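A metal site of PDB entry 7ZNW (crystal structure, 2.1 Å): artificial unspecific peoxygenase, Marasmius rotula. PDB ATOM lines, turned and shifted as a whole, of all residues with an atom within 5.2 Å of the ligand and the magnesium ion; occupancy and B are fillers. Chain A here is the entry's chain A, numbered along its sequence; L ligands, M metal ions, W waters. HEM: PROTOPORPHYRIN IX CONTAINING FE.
Water W3 lies within hydrogen-bond range of the backbone carbonyl oxygen (O) of Asn 107 (2.9 Å) and an oxygen (O2D) of the ligand (3.4 Å).
Water W4 bridges OE1 of Glu 164 (2.6 Å) and O2A of the ligand (2.7 Å).
Water W2 bridges O of Pro 23 and O2D of the ligand.
Of the 33 residues printed, 3 come within 4 Å of the magnesium ion.
Along chain A the residues within 4 Å of the magnesium ion span positions 92 to 96.
The nearest printed residue that does not touch the magnesium ion is Asp 94 (4.3 Å).
Residues that only touch the ligand: Glu 164 (3.2 Å), Leu 85 (3.4 Å), Ile 91 (3.4 Å), Leu 27 (3.5 Å), Leu 63 (3.5 Å), Ala 66 (3.6 Å), Ile 48 (3.6 Å), Phe 167 (3.6 Å), Ala 67 (3.6 Å), Pro 25 (3.7 Å), Gly 26 (3.7 Å), Pro 23 (3.7 Å), Phe 80 (3.7 Å), Val 171 (3.8 Å), Tyr 56 (3.9 Å), Phe 189 (3.95 Å) and Arg 99 (3.96 Å).
Hydrophobic or aromatic side chains that line the ligand: Pro 23, Pro 25, Leu 27, Ile 48, Tyr 56, Leu 63, Ala 66, Phe 80, Ile 91, His 93, Leu 97, Phe 167, Val 171 and Phe 189.
Within 4 Å of the ligand: Pro 23, Cys 24, Pro 25, Gly 26, Leu 27, Ile 48, Tyr 56, Leu 63, Ala 66, Ala 67, Phe 80, Leu 85, Ile 91, Glu 92, His 93, Ser 96, Leu 97, Ser 98, Arg 99, Glu 164, Phe 167, Val 171 and Phe 189.
The nearest printed residue that does not touch the ligand is Tyr 168 (4.1 Å).
The magnesium ion is bound by OG of Ser 96 (2.1 Å), water W3 (2.1 Å), water W5 (2.1 Å), OE2 of Glu 92 (2.1 Å), O of His 93 (2.1 Å) and O1D of the ligand (2.2 Å).
The magnesium ion has six donor atoms within binding distance.
The backbone NH (N) of His 93 lies close to an oxygen (O1D) of the ligand (2.7 Å).
NE2 of His 93 lies close to O2D of the ligand (3.4 Å).
The side-chain sulfur (SG) of Cys 24 binds an iron atom (FE) of the ligand, 2.3 Å away.
The backbone NH (N) of Ser 98 is in hydrogen-bond range of an oxygen (O1A) of the ligand (2.8 Å).
The side-chain hydroxyl (OG) of Ser 98 is in hydrogen-bond range of an oxygen (O1A) of the ligand (2.7 Å).
N of Leu 97 is in hydrogen-bond range of O2A of the ligand (2.8 Å).
OE1 of Glu 92 is in hydrogen-bond range of ND2 of Asn 107 (2.8 Å).
A ring nitrogen (NE2) of His 93 lies within hydrogen-bond range of the side-chain carboxylate of Glu 164, at 2.5 Å.
The backbone NH of Leu 27 lies close to the side-chain sulfur of Cys 24 (3.3 Å).
The side-chain sulfur (SG) of Cys 24 sits close to the backbone NH (N) of Gly 26 (3.2 Å).
OG of Ser 98 is in hydrogen-bond range of NH1 of Arg 99 (2.9 Å).
The backbone carbonyl oxygen (O) of Gly 26 lies within hydrogen-bond range of the side-chain hydroxyl (OH) of Tyr 56 (2.6 Å).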
ATOM      1  N   PRO A  23     -17.530 -18.990 -17.062  1.00  0.00           N
ATOM      2  CA  PRO A  23     -16.980 -19.117 -15.717  1.00  0.00           C
ATOM      3  C   PRO A  23     -17.965 -19.791 -14.735  1.00  0.00           C
ATOM      4  O   PRO A  23     -17.667 -19.804 -13.546  1.00  0.00           O
ATOM      5  CB  PRO A  23     -16.725 -17.662 -15.285  1.00  0.00           C
ATOM      6  CG  PRO A  23     -17.139 -16.793 -16.462  1.00  0.00           C
ATOM      7  CD  PRO A  23     -18.054 -17.647 -17.306  1.00  0.00           C
ATOM      8  N   CYS A  24     -19.076 -20.312 -15.253  1.00  0.00           N
ATOM      9  CA  CYS A  24     -20.149 -20.892 -14.413  1.00  0.00           C
ATOM     10  C   CYS A  24     -20.158 -22.422 -14.514  1.00  0.00           C
ATOM     11  O   CYS A  24     -20.578 -22.924 -15.561  1.00  0.00           O
ATOM     12  CB  CYS A  24     -21.520 -20.373 -14.819  1.00  0.00           C
ATOM     13  SG  CYS A  24     -22.867 -21.157 -13.917  1.00  0.00           S
ATOM     14  N   PRO A  25     -19.792 -23.172 -13.454  1.00  0.00           N
ATOM     15  CA  PRO A  25     -19.885 -24.624 -13.493  1.00  0.00           C
ATOM     16  C   PRO A  25     -21.325 -25.075 -13.721  1.00  0.00           C
ATOM     17  O   PRO A  25     -21.508 -26.121 -14.290  1.00  0.00           O
ATOM     18  CB  PRO A  25     -19.344 -25.069 -12.117  1.00  0.00           C
ATOM     19  CG  PRO A  25     -19.558 -23.847 -11.233  1.00  0.00           C
ATOM     20  CD  PRO A  25     -19.293 -22.685 -12.163  1.00  0.00           C
ATOM     21  N   GLY A  26     -22.322 -24.287 -13.275  1.00  0.00           N
ATOM     22  CA  GLY A  26     -23.736 -24.663 -13.453  1.00  0.00           C
ATOM     23  C   GLY A  26     -24.097 -24.815 -14.916  1.00  0.00           C
ATOM     24  O   GLY A  26     -24.546 -25.898 -15.322  1.00  0.00           O
ATOM     25  N   LEU A  27     -23.859 -23.776 -15.723  1.00  0.00           N
ATOM     26  CA  LEU A  27     -24.176 -23.788 -17.160  1.00  0.00           C
ATOM     27  C   LEU A  27     -23.224 -24.715 -17.899  1.00  0.00           C
ATOM     28  O   LEU A  27     -23.701 -25.426 -18.801  1.00  0.00           O
ATOM     29  CB  LEU A  27     -24.110 -22.357 -17.705  1.00  0.00           C
ATOM     30  CG  LEU A  27     -25.079 -21.359 -17.061  1.00  0.00           C
ATOM     31  CD1 LEU A  27     -25.019 -20.027 -17.813  1.00  0.00           C
ATOM     32  CD2 LEU A  27     -26.498 -21.910 -17.010  1.00  0.00           C
ATOM     33  N   LEU A  30     -24.397 -28.224 -17.557  1.00  0.00           N
ATOM     34  CA  LEU A  30     -25.617 -28.398 -18.407  1.00  0.00           C
ATOM     35  C   LEU A  30     -25.190 -28.550 -19.886  1.00  0.00           C
ATOM     36  O   LEU A  30     -25.719 -29.457 -20.541  1.00  0.00           O
ATOM     37  CB  LEU A  30     -26.560 -27.220 -18.202  1.00  0.00           C
ATOM     38  CG  LEU A  30     -27.285 -27.172 -16.850  1.00  0.00           C
ATOM     39  CD1 LEU A  30     -28.103 -25.899 -16.691  1.00  0.00           C
ATOM     40  CD2 LEU A  30     -28.174 -28.381 -16.664  1.00  0.00           C
ATOM     41  N   ILE A  48     -32.210 -21.529 -21.180  1.00  0.00           N
ATOM     42  CA  ILE A  48     -31.656 -21.506 -19.790  1.00  0.00           C
ATOM     43  C   ILE A  48     -32.703 -22.057 -18.787  1.00  0.00           C
ATOM     44  O   ILE A  48     -32.315 -22.895 -17.975  1.00  0.00           O
ATOM     45  CB  ILE A  48     -31.146 -20.108 -19.387  1.00  0.00           C
ATOM     46  CG1 ILE A  48     -29.946 -19.714 -20.252  1.00  0.00           C
ATOM     47  CG2 ILE A  48     -30.810 -20.063 -17.903  1.00  0.00           C
ATOM     48  CD1 ILE A  48     -28.637 -20.401 -19.853  1.00  0.00           C
ATOM     49  N   GLY A  52     -32.057 -25.557 -16.781  1.00  0.00           N
ATOM     50  CA  GLY A  52     -31.965 -25.443 -15.314  1.00  0.00           C
ATOM     51  C   GLY A  52     -32.994 -26.324 -14.612  1.00  0.00           C
ATOM     52  O   GLY A  52     -32.637 -27.004 -13.606  1.00  0.00           O
ATOM     53  N   TYR A  56     -31.363 -29.703 -12.872  1.00  0.00           N
ATOM     54  CA  TYR A  56     -31.127 -29.417 -11.442  1.00  0.00           C
ATOM     55  C   TYR A  56     -32.444 -29.252 -10.660  1.00  0.00           C
ATOM     56  O   TYR A  56     -32.365 -29.119  -9.407  1.00  0.00           O
ATOM     57  CB  TYR A  56     -30.314 -28.130 -11.275  1.00  0.00           C
ATOM     58  CG  TYR A  56     -28.966 -28.073 -11.946  1.00  0.00           C
ATOM     59  CD1 TYR A  56     -28.036 -29.088 -11.781  1.00  0.00           C
ATOM     60  CD2 TYR A  56     -28.590 -26.962 -12.698  1.00  0.00           C
ATOM     61  CE1 TYR A  56     -26.765 -29.006 -12.348  1.00  0.00           C
ATOM     62  CE2 TYR A  56     -27.320 -26.866 -13.263  1.00  0.00           C
ATOM     63  CZ  TYR A  56     -26.409 -27.891 -13.091  1.00  0.00           C
ATOM     64  OH  TYR A  56     -25.160 -27.828 -13.643  1.00  0.00           O
ATOM     65  N   VAL A  58     -34.046 -26.509 -10.861  1.00  0.00           N
ATOM     66  CA  VAL A  58     -34.070 -25.060 -10.506  1.00  0.00           C
ATOM     67  C   VAL A  58     -35.263 -24.409 -11.247  1.00  0.00           C
ATOM     68  O   VAL A  58     -35.415 -24.637 -12.471  1.00  0.00           O
ATOM     69  CB  VAL A  58     -32.725 -24.367 -10.780  1.00  0.00           C
ATOM     70  CG1 VAL A  58     -32.833 -22.872 -10.542  1.00  0.00           C
ATOM     71  CG2 VAL A  58     -31.620 -24.940  -9.916  1.00  0.00           C
ATOM     72  N   LEU A  63     -33.511 -18.165 -12.627  1.00  0.00           N
ATOM     73  CA  LEU A  63     -32.854 -18.359 -13.956  1.00  0.00           C
ATOM     74  C   LEU A  63     -33.160 -17.219 -14.936  1.00  0.00           C
ATOM     75  O   LEU A  63     -32.248 -16.811 -15.713  1.00  0.00           O
ATOM     76  CB  LEU A  63     -33.281 -19.708 -14.530  1.00  0.00           C
ATOM     77  CG  LEU A  63     -32.822 -20.911 -13.700  1.00  0.00           C
ATOM     78  CD1 LEU A  63     -33.431 -22.198 -14.223  1.00  0.00           C
ATOM     79  CD2 LEU A  63     -31.307 -21.003 -13.685  1.00  0.00           C
ATOM     80  N   ALA A  66     -31.035 -14.101 -13.953  1.00  0.00           N
ATOM     81  CA  ALA A  66     -29.607 -14.323 -14.213  1.00  0.00           C
ATOM     82  C   ALA A  66     -29.385 -14.269 -15.736  1.00  0.00           C
ATOM     83  O   ALA A  66     -28.420 -13.656 -16.194  1.00  0.00           O
ATOM     84  CB  ALA A  66     -29.142 -15.631 -13.591  1.00  0.00           C
ATOM     85  N   ALA A  67     -30.255 -14.907 -16.502  1.00  0.00           N
ATOM     86  CA  ALA A  67     -30.110 -15.000 -17.966  1.00  0.00           C
ATOM     87  C   ALA A  67     -30.302 -13.621 -18.608  1.00  0.00           C
ATOM     88  O   ALA A  67     -29.593 -13.291 -19.582  1.00  0.00           O
ATOM     89  CB  ALA A  67     -31.075 -16.015 -18.520  1.00  0.00           C
ATOM     90  N   GLY A  70     -27.127 -11.904 -18.046  1.00  0.00           N
ATOM     91  CA  GLY A  70     -26.175 -12.600 -18.942  1.00  0.00           C
ATOM     92  C   GLY A  70     -26.269 -12.077 -20.368  1.00  0.00           C
ATOM     93  O   GLY A  70     -25.193 -11.907 -21.032  1.00  0.00           O
ATOM     94  N   PHE A  80     -26.889 -15.371 -26.137  1.00  0.00           N
ATOM     95  CA  PHE A  80     -25.480 -15.239 -25.685  1.00  0.00           C
ATOM     96  C   PHE A  80     -24.829 -16.603 -25.876  1.00  0.00           C
ATOM     97  O   PHE A  80     -25.528 -17.635 -25.999  1.00  0.00           O
ATOM     98  CB  PHE A  80     -25.372 -14.725 -24.251  1.00  0.00           C
ATOM     99  CG  PHE A  80     -26.074 -15.558 -23.199  1.00  0.00           C
ATOM    100  CD1 PHE A  80     -25.505 -16.719 -22.698  1.00  0.00           C
ATOM    101  CD2 PHE A  80     -27.280 -15.133 -22.656  1.00  0.00           C
ATOM    102  CE1 PHE A  80     -26.153 -17.463 -21.716  1.00  0.00           C
ATOM    103  CE2 PHE A  80     -27.919 -15.864 -21.660  1.00  0.00           C
ATOM    104  CZ  PHE A  80     -27.359 -17.037 -21.203  1.00  0.00           C
ATOM    105  N   LEU A  85     -20.275 -14.741 -21.174  1.00  0.00           N
ATOM    106  CA  LEU A  85     -20.616 -14.550 -19.726  1.00  0.00           C
ATOM    107  C   LEU A  85     -19.361 -14.179 -18.907  1.00  0.00           C
ATOM    108  O   LEU A  85     -19.530 -13.755 -17.759  1.00  0.00           O
ATOM    109  CB  LEU A  85     -21.250 -15.849 -19.202  1.00  0.00           C
ATOM    110  CG  LEU A  85     -22.575 -16.223 -19.853  1.00  0.00           C
ATOM    111  CD1 LEU A  85     -23.069 -17.561 -19.299  1.00  0.00           C
ATOM    112  CD2 LEU A  85     -23.601 -15.113 -19.683  1.00  0.00           C
ATOM    113  N   ILE A  91     -21.944 -10.126 -14.426  1.00  0.00           N
ATOM    114  CA  ILE A  91     -22.032 -11.138 -13.327  1.00  0.00           C
ATOM    115  C   ILE A  91     -20.615 -11.469 -12.849  1.00  0.00           C
ATOM    116  O   ILE A  91     -20.383 -11.419 -11.626  1.00  0.00           O
ATOM    117  CB  ILE A  91     -22.784 -12.386 -13.819  1.00  0.00           C
ATOM    118  CG1 ILE A  91     -24.229 -12.055 -14.205  1.00  0.00           C
ATOM    119  CG2 ILE A  91     -22.741 -13.497 -12.780  1.00  0.00           C
ATOM    120  CD1 ILE A  91     -24.918 -13.151 -14.974  1.00  0.00           C
ATOM    121  N   GLU A  92     -19.699 -11.787 -13.782  1.00  0.00           N
ATOM    122  CA  GLU A  92     -18.340 -12.273 -13.427  1.00  0.00           C
ATOM    123  C   GLU A  92     -17.722 -11.245 -12.463  1.00  0.00           C
ATOM    124  O   GLU A  92     -17.832 -10.016 -12.689  1.00  0.00           O
ATOM    125  CB  GLU A  92     -17.502 -12.558 -14.677  1.00  0.00           C
ATOM    126  CG  GLU A  92     -16.240 -13.327 -14.338  1.00  0.00           C
ATOM    127  CD  GLU A  92     -15.165 -12.479 -13.667  1.00  0.00           C
ATOM    128  OE1 GLU A  92     -15.064 -11.284 -14.031  1.00  0.00           O
ATOM    129  OE2 GLU A  92     -14.442 -12.989 -12.783  1.00  0.00           O
ATOM    130  N   HIS A  93     -17.183 -11.767 -11.359  1.00  0.00           N
ATOM    131  CA  HIS A  93     -16.704 -10.953 -10.208  1.00  0.00           C
ATOM    132  C   HIS A  93     -15.378 -11.513  -9.693  1.00  0.00           C
ATOM    133  O   HIS A  93     -15.060 -12.707  -9.916  1.00  0.00           O
ATOM    134  CB  HIS A  93     -17.772 -10.931  -9.110  1.00  0.00           C
ATOM    135  CG  HIS A  93     -18.162 -12.321  -8.698  1.00  0.00           C
ATOM    136  ND1 HIS A  93     -17.299 -13.164  -7.987  1.00  0.00           N
ATOM    137  CD2 HIS A  93     -19.266 -13.050  -8.965  1.00  0.00           C
ATOM    138  CE1 HIS A  93     -17.868 -14.337  -7.822  1.00  0.00           C
ATOM    139  NE2 HIS A  93     -19.095 -14.299  -8.422  1.00  0.00           N
ATOM    140  N   ASP A  94     -14.647 -10.666  -8.972  1.00  0.00           N
ATOM    141  CA  ASP A  94     -13.453 -11.030  -8.185  1.00  0.00           C
ATOM    142  C   ASP A  94     -13.849 -12.007  -7.062  1.00  0.00           C
ATOM    143  O   ASP A  94     -15.049 -12.045  -6.713  1.00  0.00           O
ATOM    144  CB  ASP A  94     -12.783  -9.746  -7.670  1.00  0.00           C
ATOM    145  CG  ASP A  94     -12.348  -8.857  -8.817  1.00  0.00           C
ATOM    146  OD1 ASP A  94     -12.080  -9.426  -9.919  1.00  0.00           O
ATOM    147  OD2 ASP A  94     -12.324  -7.607  -8.631  1.00  0.00           O
ATOM    148  N   SER A  96     -13.881 -15.348  -6.981  1.00  0.00           N
ATOM    149  CA  SER A  96     -14.567 -16.570  -7.451  1.00  0.00           C
ATOM    150  C   SER A  96     -13.986 -17.753  -6.660  1.00  0.00           C
ATOM    151  O   SER A  96     -12.858 -17.628  -6.149  1.00  0.00           O
ATOM    152  CB  SER A  96     -14.423 -16.792  -8.950  1.00  0.00           C
ATOM    153  OG  SER A  96     -15.010 -15.748  -9.706  1.00  0.00           O
ATOM    154  N   LEU A  97     -14.724 -18.850  -6.626  1.00  0.00           N
ATOM    155  CA  LEU A  97     -14.358 -20.097  -5.933  1.00  0.00           C
ATOM    156  C   LEU A  97     -13.311 -20.882  -6.710  1.00  0.00           C
ATOM    157  O   LEU A  97     -12.566 -21.641  -6.069  1.00  0.00           O
ATOM    158  CB  LEU A  97     -15.632 -20.923  -5.768  1.00  0.00           C
ATOM    159  CG  LEU A  97     -16.754 -20.258  -4.985  1.00  0.00           C
ATOM    160  CD1 LEU A  97     -18.020 -21.070  -5.103  1.00  0.00           C
ATOM    161  CD2 LEU A  97     -16.377 -20.092  -3.514  1.00  0.00           C
ATOM    162  N   SER A  98     -13.319 -20.806  -8.043  1.00  0.00           N
ATOM    163  CA  SER A  98     -12.508 -21.715  -8.911  1.00  0.00           C
ATOM    164  C   SER A  98     -11.855 -20.970 -10.090  1.00  0.00           C
ATOM    165  O   SER A  98     -11.245 -21.656 -10.917  1.00  0.00           O
ATOM    166  CB  SER A  98     -13.370 -22.842  -9.406  1.00  0.00           C
ATOM    167  OG  SER A  98     -14.392 -22.349 -10.255  1.00  0.00           O
ATOM    168  N   ARG A  99     -11.960 -19.651 -10.101  1.00  0.00           N
ATOM    169  CA  ARG A  99     -11.368 -18.841 -11.193  1.00  0.00           C
ATOM    170  C   ARG A  99     -10.528 -17.695 -10.626  1.00  0.00           C
ATOM    171  O   ARG A  99     -10.876 -17.210  -9.546  1.00  0.00           O
ATOM    172  CB  ARG A  99     -12.488 -18.296 -12.097  1.00  0.00           C
ATOM    173  CG  ARG A  99     -12.796 -19.153 -13.324  1.00  0.00           C
ATOM    174  CD  ARG A  99     -13.557 -20.414 -12.986  1.00  0.00           C
ATOM    175  NE  ARG A  99     -14.135 -21.046 -14.157  1.00  0.00           N
ATOM    176  CZ  ARG A  99     -14.699 -22.245 -14.165  1.00  0.00           C
ATOM    177  NH1 ARG A  99     -14.765 -22.948 -13.053  1.00  0.00           N
ATOM    178  NH2 ARG A  99     -15.197 -22.726 -15.282  1.00  0.00           N
ATOM    179  N   GLU A 100      -9.454 -17.309 -11.313  1.00  0.00           N
ATOM    180  CA  GLU A 100      -8.641 -16.124 -10.954  1.00  0.00           C
ATOM    181  C   GLU A 100      -9.480 -14.866 -11.183  1.00  0.00           C
ATOM    182  O   GLU A 100     -10.424 -14.880 -12.028  1.00  0.00           O
ATOM    183  CB  GLU A 100      -7.341 -16.036 -11.768  1.00  0.00           C
ATOM    184  CG  GLU A 100      -6.486 -17.288 -11.659  1.00  0.00           C
ATOM    185  CD  GLU A 100      -5.246 -17.299 -12.553  1.00  0.00           C
ATOM    186  OE1 GLU A 100      -5.297 -16.806 -13.717  1.00  0.00           O
ATOM    187  OE2 GLU A 100      -4.228 -17.807 -12.088  1.00  0.00           O
ATOM    188  N   ASN A 107     -10.133 -15.148 -15.743  1.00  0.00           N
ATOM    189  CA  ASN A 107     -11.424 -15.153 -15.007  1.00  0.00           C
ATOM    190  C   ASN A 107     -12.423 -16.137 -15.639  1.00  0.00           C
ATOM    191  O   ASN A 107     -13.617 -16.122 -15.237  1.00  0.00           O
ATOM    192  CB  ASN A 107     -11.994 -13.725 -14.954  1.00  0.00           C
ATOM    193  CG  ASN A 107     -12.631 -13.264 -16.250  1.00  0.00           C
ATOM    194  OD1 ASN A 107     -12.410 -13.812 -17.324  1.00  0.00           O
ATOM    195  ND2 ASN A 107     -13.447 -12.229 -16.168  1.00  0.00           N
ATOM    196  N   GLU A 164     -24.213 -17.873  -5.531  1.00  0.00           N
ATOM    197  CA  GLU A 164     -23.460 -18.895  -6.293  1.00  0.00           C
ATOM    198  C   GLU A 164     -23.063 -20.032  -5.347  1.00  0.00           C
ATOM    199  O   GLU A 164     -23.138 -21.203  -5.759  1.00  0.00           O
ATOM    200  CB  GLU A 164     -22.285 -18.242  -7.027  1.00  0.00           C
ATOM    201  CG  GLU A 164     -22.734 -17.306  -8.149  1.00  0.00           C
ATOM    202  CD  GLU A 164     -21.639 -16.429  -8.729  1.00  0.00           C
ATOM    203  OE1 GLU A 164     -20.555 -16.243  -8.052  1.00  0.00           O
ATOM    204  OE2 GLU A 164     -21.824 -15.960  -9.901  1.00  0.00           O
ATOM    205  N   SER A 165     -22.705 -19.692  -4.103  1.00  0.00           N
ATOM    206  CA  SER A 165     -22.330 -20.680  -3.049  1.00  0.00           C
ATOM    207  C   SER A 165     -23.589 -21.449  -2.618  1.00  0.00           C
ATOM    208  O   SER A 165     -23.512 -22.689  -2.479  1.00  0.00           O
ATOM    209  CB  SER A 165     -21.618 -20.034  -1.919  1.00  0.00           C
ATOM    210  OG  SER A 165     -20.271 -19.831  -2.272  1.00  0.00           O
ATOM    211  N   PHE A 167     -25.936 -22.034  -4.631  1.00  0.00           N
ATOM    212  CA  PHE A 167     -26.219 -22.879  -5.811  1.00  0.00           C
ATOM    213  C   PHE A 167     -25.452 -24.204  -5.714  1.00  0.00           C
ATOM    214  O   PHE A 167     -26.098 -25.251  -5.888  1.00  0.00           O
ATOM    215  CB  PHE A 167     -25.902 -22.166  -7.127  1.00  0.00           C
ATOM    216  CG  PHE A 167     -27.115 -21.615  -7.840  1.00  0.00           C
ATOM    217  CD1 PHE A 167     -28.259 -22.380  -7.992  1.00  0.00           C
ATOM    218  CD2 PHE A 167     -27.077 -20.339  -8.382  1.00  0.00           C
ATOM    219  CE1 PHE A 167     -29.353 -21.887  -8.690  1.00  0.00           C
ATOM    220  CE2 PHE A 167     -28.170 -19.860  -9.083  1.00  0.00           C
ATOM    221  CZ  PHE A 167     -29.308 -20.622  -9.210  1.00  0.00           C
ATOM    222  N   TYR A 168     -24.146 -24.189  -5.462  1.00  0.00           N
ATOM    223  CA  TYR A 168     -23.362 -25.457  -5.455  1.00  0.00           C
ATOM    224  C   TYR A 168     -23.871 -26.360  -4.321  1.00  0.00           C
ATOM    225  O   TYR A 168     -24.081 -27.579  -4.545  1.00  0.00           O
ATOM    226  CB  TYR A 168     -21.842 -25.199  -5.482  1.00  0.00           C
ATOM    227  CG  TYR A 168     -21.114 -24.836  -4.221  1.00  0.00           C
ATOM    228  CD1 TYR A 168     -20.930 -25.733  -3.179  1.00  0.00           C
ATOM    229  CD2 TYR A 168     -20.516 -23.590  -4.098  1.00  0.00           C
ATOM    230  CE1 TYR A 168     -20.216 -25.396  -2.035  1.00  0.00           C
ATOM    231  CE2 TYR A 168     -19.792 -23.241  -2.970  1.00  0.00           C
ATOM    232  CZ  TYR A 168     -19.657 -24.141  -1.924  1.00  0.00           C
ATOM    233  OH  TYR A 168     -18.937 -23.771  -0.826  1.00  0.00           O
ATOM    234  N   VAL A 171     -27.719 -27.583  -5.621  1.00  0.00           N
ATOM    235  CA  VAL A 171     -27.961 -28.455  -6.806  1.00  0.00           C
ATOM    236  C   VAL A 171     -27.206 -29.776  -6.629  1.00  0.00           C
ATOM    237  O   VAL A 171     -27.703 -30.791  -7.151  1.00  0.00           O
ATOM    238  CB  VAL A 171     -27.617 -27.768  -8.160  1.00  0.00           C
ATOM    239  CG1 VAL A 171     -28.338 -26.434  -8.325  1.00  0.00           C
ATOM    240  CG2 VAL A 171     -26.127 -27.600  -8.370  1.00  0.00           C
ATOM    241  N   PHE A 188     -18.429 -31.653  -9.875  1.00  0.00           N
ATOM    242  CA  PHE A 188     -19.137 -30.492 -10.461  1.00  0.00           C
ATOM    243  C   PHE A 188     -18.122 -29.443 -10.916  1.00  0.00           C
ATOM    244  O   PHE A 188     -18.121 -29.070 -12.083  1.00  0.00           O
ATOM    245  CB  PHE A 188     -20.128 -29.955  -9.417  1.00  0.00           C
ATOM    246  CG  PHE A 188     -20.996 -28.801  -9.833  1.00  0.00           C
ATOM    247  CD1 PHE A 188     -21.907 -28.926 -10.855  1.00  0.00           C
ATOM    248  CD2 PHE A 188     -20.957 -27.613  -9.114  1.00  0.00           C
ATOM    249  CE1 PHE A 188     -22.723 -27.855 -11.217  1.00  0.00           C
ATOM    250  CE2 PHE A 188     -21.788 -26.559  -9.467  1.00  0.00           C
ATOM    251  CZ  PHE A 188     -22.664 -26.685 -10.511  1.00  0.00           C
ATOM    252  N   PHE A 189     -17.212 -29.018 -10.035  1.00  0.00           N
ATOM    253  CA  PHE A 189     -16.251 -27.928 -10.357  1.00  0.00           C
ATOM    254  C   PHE A 189     -15.135 -28.431 -11.276  1.00  0.00           C
ATOM    255  O   PHE A 189     -14.799 -27.737 -12.247  1.00  0.00           O
ATOM    256  CB  PHE A 189     -15.688 -27.292  -9.076  1.00  0.00           C
ATOM    257  CG  PHE A 189     -16.524 -26.211  -8.458  1.00  0.00           C
ATOM    258  CD1 PHE A 189     -16.349 -24.883  -8.824  1.00  0.00           C
ATOM    259  CD2 PHE A 189     -17.468 -26.512  -7.487  1.00  0.00           C
ATOM    260  CE1 PHE A 189     -17.111 -23.891  -8.252  1.00  0.00           C
ATOM    261  CE2 PHE A 189     -18.226 -25.500  -6.905  1.00  0.00           C
ATOM    262  CZ  PHE A 189     -18.052 -24.195  -7.294  1.00  0.00           C
HETATM  263  CHA HEM L   1     -20.630 -18.490 -11.404  1.00  0.00           C
HETATM  264  CHB HEM L   1     -23.630 -22.123 -10.330  1.00  0.00           C
HETATM  265  CHC HEM L   1     -26.893 -20.410 -13.498  1.00  0.00           C
HETATM  266  CHD HEM L   1     -23.634 -17.145 -14.897  1.00  0.00           C
HETATM  267  C1A HEM L   1     -21.242 -19.565 -10.779  1.00  0.00           C
HETATM  268  C2A HEM L   1     -20.676 -20.237  -9.652  1.00  0.00           C
HETATM  269  C3A HEM L   1     -21.531 -21.255  -9.344  1.00  0.00           C
HETATM  270  C4A HEM L   1     -22.574 -21.240 -10.297  1.00  0.00           C
HETATM  271  CMA HEM L   1     -21.357 -22.221  -8.192  1.00  0.00           C
HETATM  272  CAA HEM L   1     -19.425 -19.869  -8.887  1.00  0.00           C
HETATM  273  CBA HEM L   1     -18.137 -20.267  -9.671  1.00  0.00           C
HETATM  274  CGA HEM L   1     -16.891 -19.755  -8.998  1.00  0.00           C
HETATM  275  O1A HEM L   1     -15.769 -20.286  -9.246  1.00  0.00           O
HETATM  276  O2A HEM L   1     -17.009 -18.787  -8.193  1.00  0.00           O
HETATM  277  C1B HEM L   1     -24.741 -21.955 -11.134  1.00  0.00           C
HETATM  278  C2B HEM L   1     -25.843 -22.851 -11.051  1.00  0.00           C
HETATM  279  C3B HEM L   1     -26.789 -22.386 -11.896  1.00  0.00           C
HETATM  280  C4B HEM L   1     -26.211 -21.177 -12.542  1.00  0.00           C
HETATM  281  CMB HEM L   1     -25.956 -24.115 -10.190  1.00  0.00           C
HETATM  282  CAB HEM L   1     -28.030 -23.095 -12.209  1.00  0.00           C
HETATM  283  CBB HEM L   1     -28.497 -23.075 -13.486  1.00  0.00           C
HETATM  284  C1C HEM L   1     -26.336 -19.340 -14.142  1.00  0.00           C
HETATM  285  C2C HEM L   1     -26.946 -18.541 -15.099  1.00  0.00           C
HETATM  286  C3C HEM L   1     -25.982 -17.609 -15.521  1.00  0.00           C
HETATM  287  C4C HEM L   1     -24.816 -17.862 -14.784  1.00  0.00           C
HETATM  288  CMC HEM L   1     -28.344 -18.714 -15.626  1.00  0.00           C
HETATM  289  CAC HEM L   1     -26.038 -16.571 -16.563  1.00  0.00           C
HETATM  290  CBC HEM L   1     -26.913 -16.649 -17.531  1.00  0.00           C
HETATM  291  C1D HEM L   1     -22.549 -17.286 -14.054  1.00  0.00           C
HETATM  292  C2D HEM L   1     -21.370 -16.405 -14.191  1.00  0.00           C
HETATM  293  C3D HEM L   1     -20.506 -16.772 -13.213  1.00  0.00           C
HETATM  294  C4D HEM L   1     -21.211 -17.863 -12.498  1.00  0.00           C
HETATM  295  CMD HEM L   1     -21.141 -15.287 -15.222  1.00  0.00           C
HETATM  296  CAD HEM L   1     -19.143 -16.122 -12.945  1.00  0.00           C
HETATM  297  CBD HEM L   1     -19.136 -15.446 -11.570  1.00  0.00           C
HETATM  298  CGD HEM L   1     -17.767 -15.457 -10.938  1.00  0.00           C
HETATM  299  O1D HEM L   1     -17.086 -14.412 -11.036  1.00  0.00           O
HETATM  300  O2D HEM L   1     -17.304 -16.471 -10.334  1.00  0.00           O
HETATM  301  NA  HEM L   1     -22.416 -20.191 -11.164  1.00  0.00           N
HETATM  302  NB  HEM L   1     -25.002 -21.009 -12.019  1.00  0.00           N
HETATM  303  NC  HEM L   1     -25.082 -18.925 -13.938  1.00  0.00           N
HETATM  304  ND  HEM L   1     -22.415 -18.131 -13.026  1.00  0.00           N
HETATM  305 FE   HEM L   1     -23.688 -19.477 -12.513  1.00  0.00          FE
HETATM  306 MG    MG M   1     -14.867 -14.378 -11.225  1.00  0.00          MG
HETATM  307  O   HOH W   1     -24.539 -18.111 -11.009  1.00  0.00           O
HETATM  308  O   HOH W   2     -16.029 -18.146 -12.174  1.00  0.00           O
HETATM  309  O   HOH W   3     -14.828 -15.895 -12.626  1.00  0.00           O
HETATM  310  O   HOH W   4     -18.647 -17.342  -6.668  1.00  0.00           O
HETATM  311  O   HOH W   5     -12.815 -14.428 -10.772  1.00  0.00           O
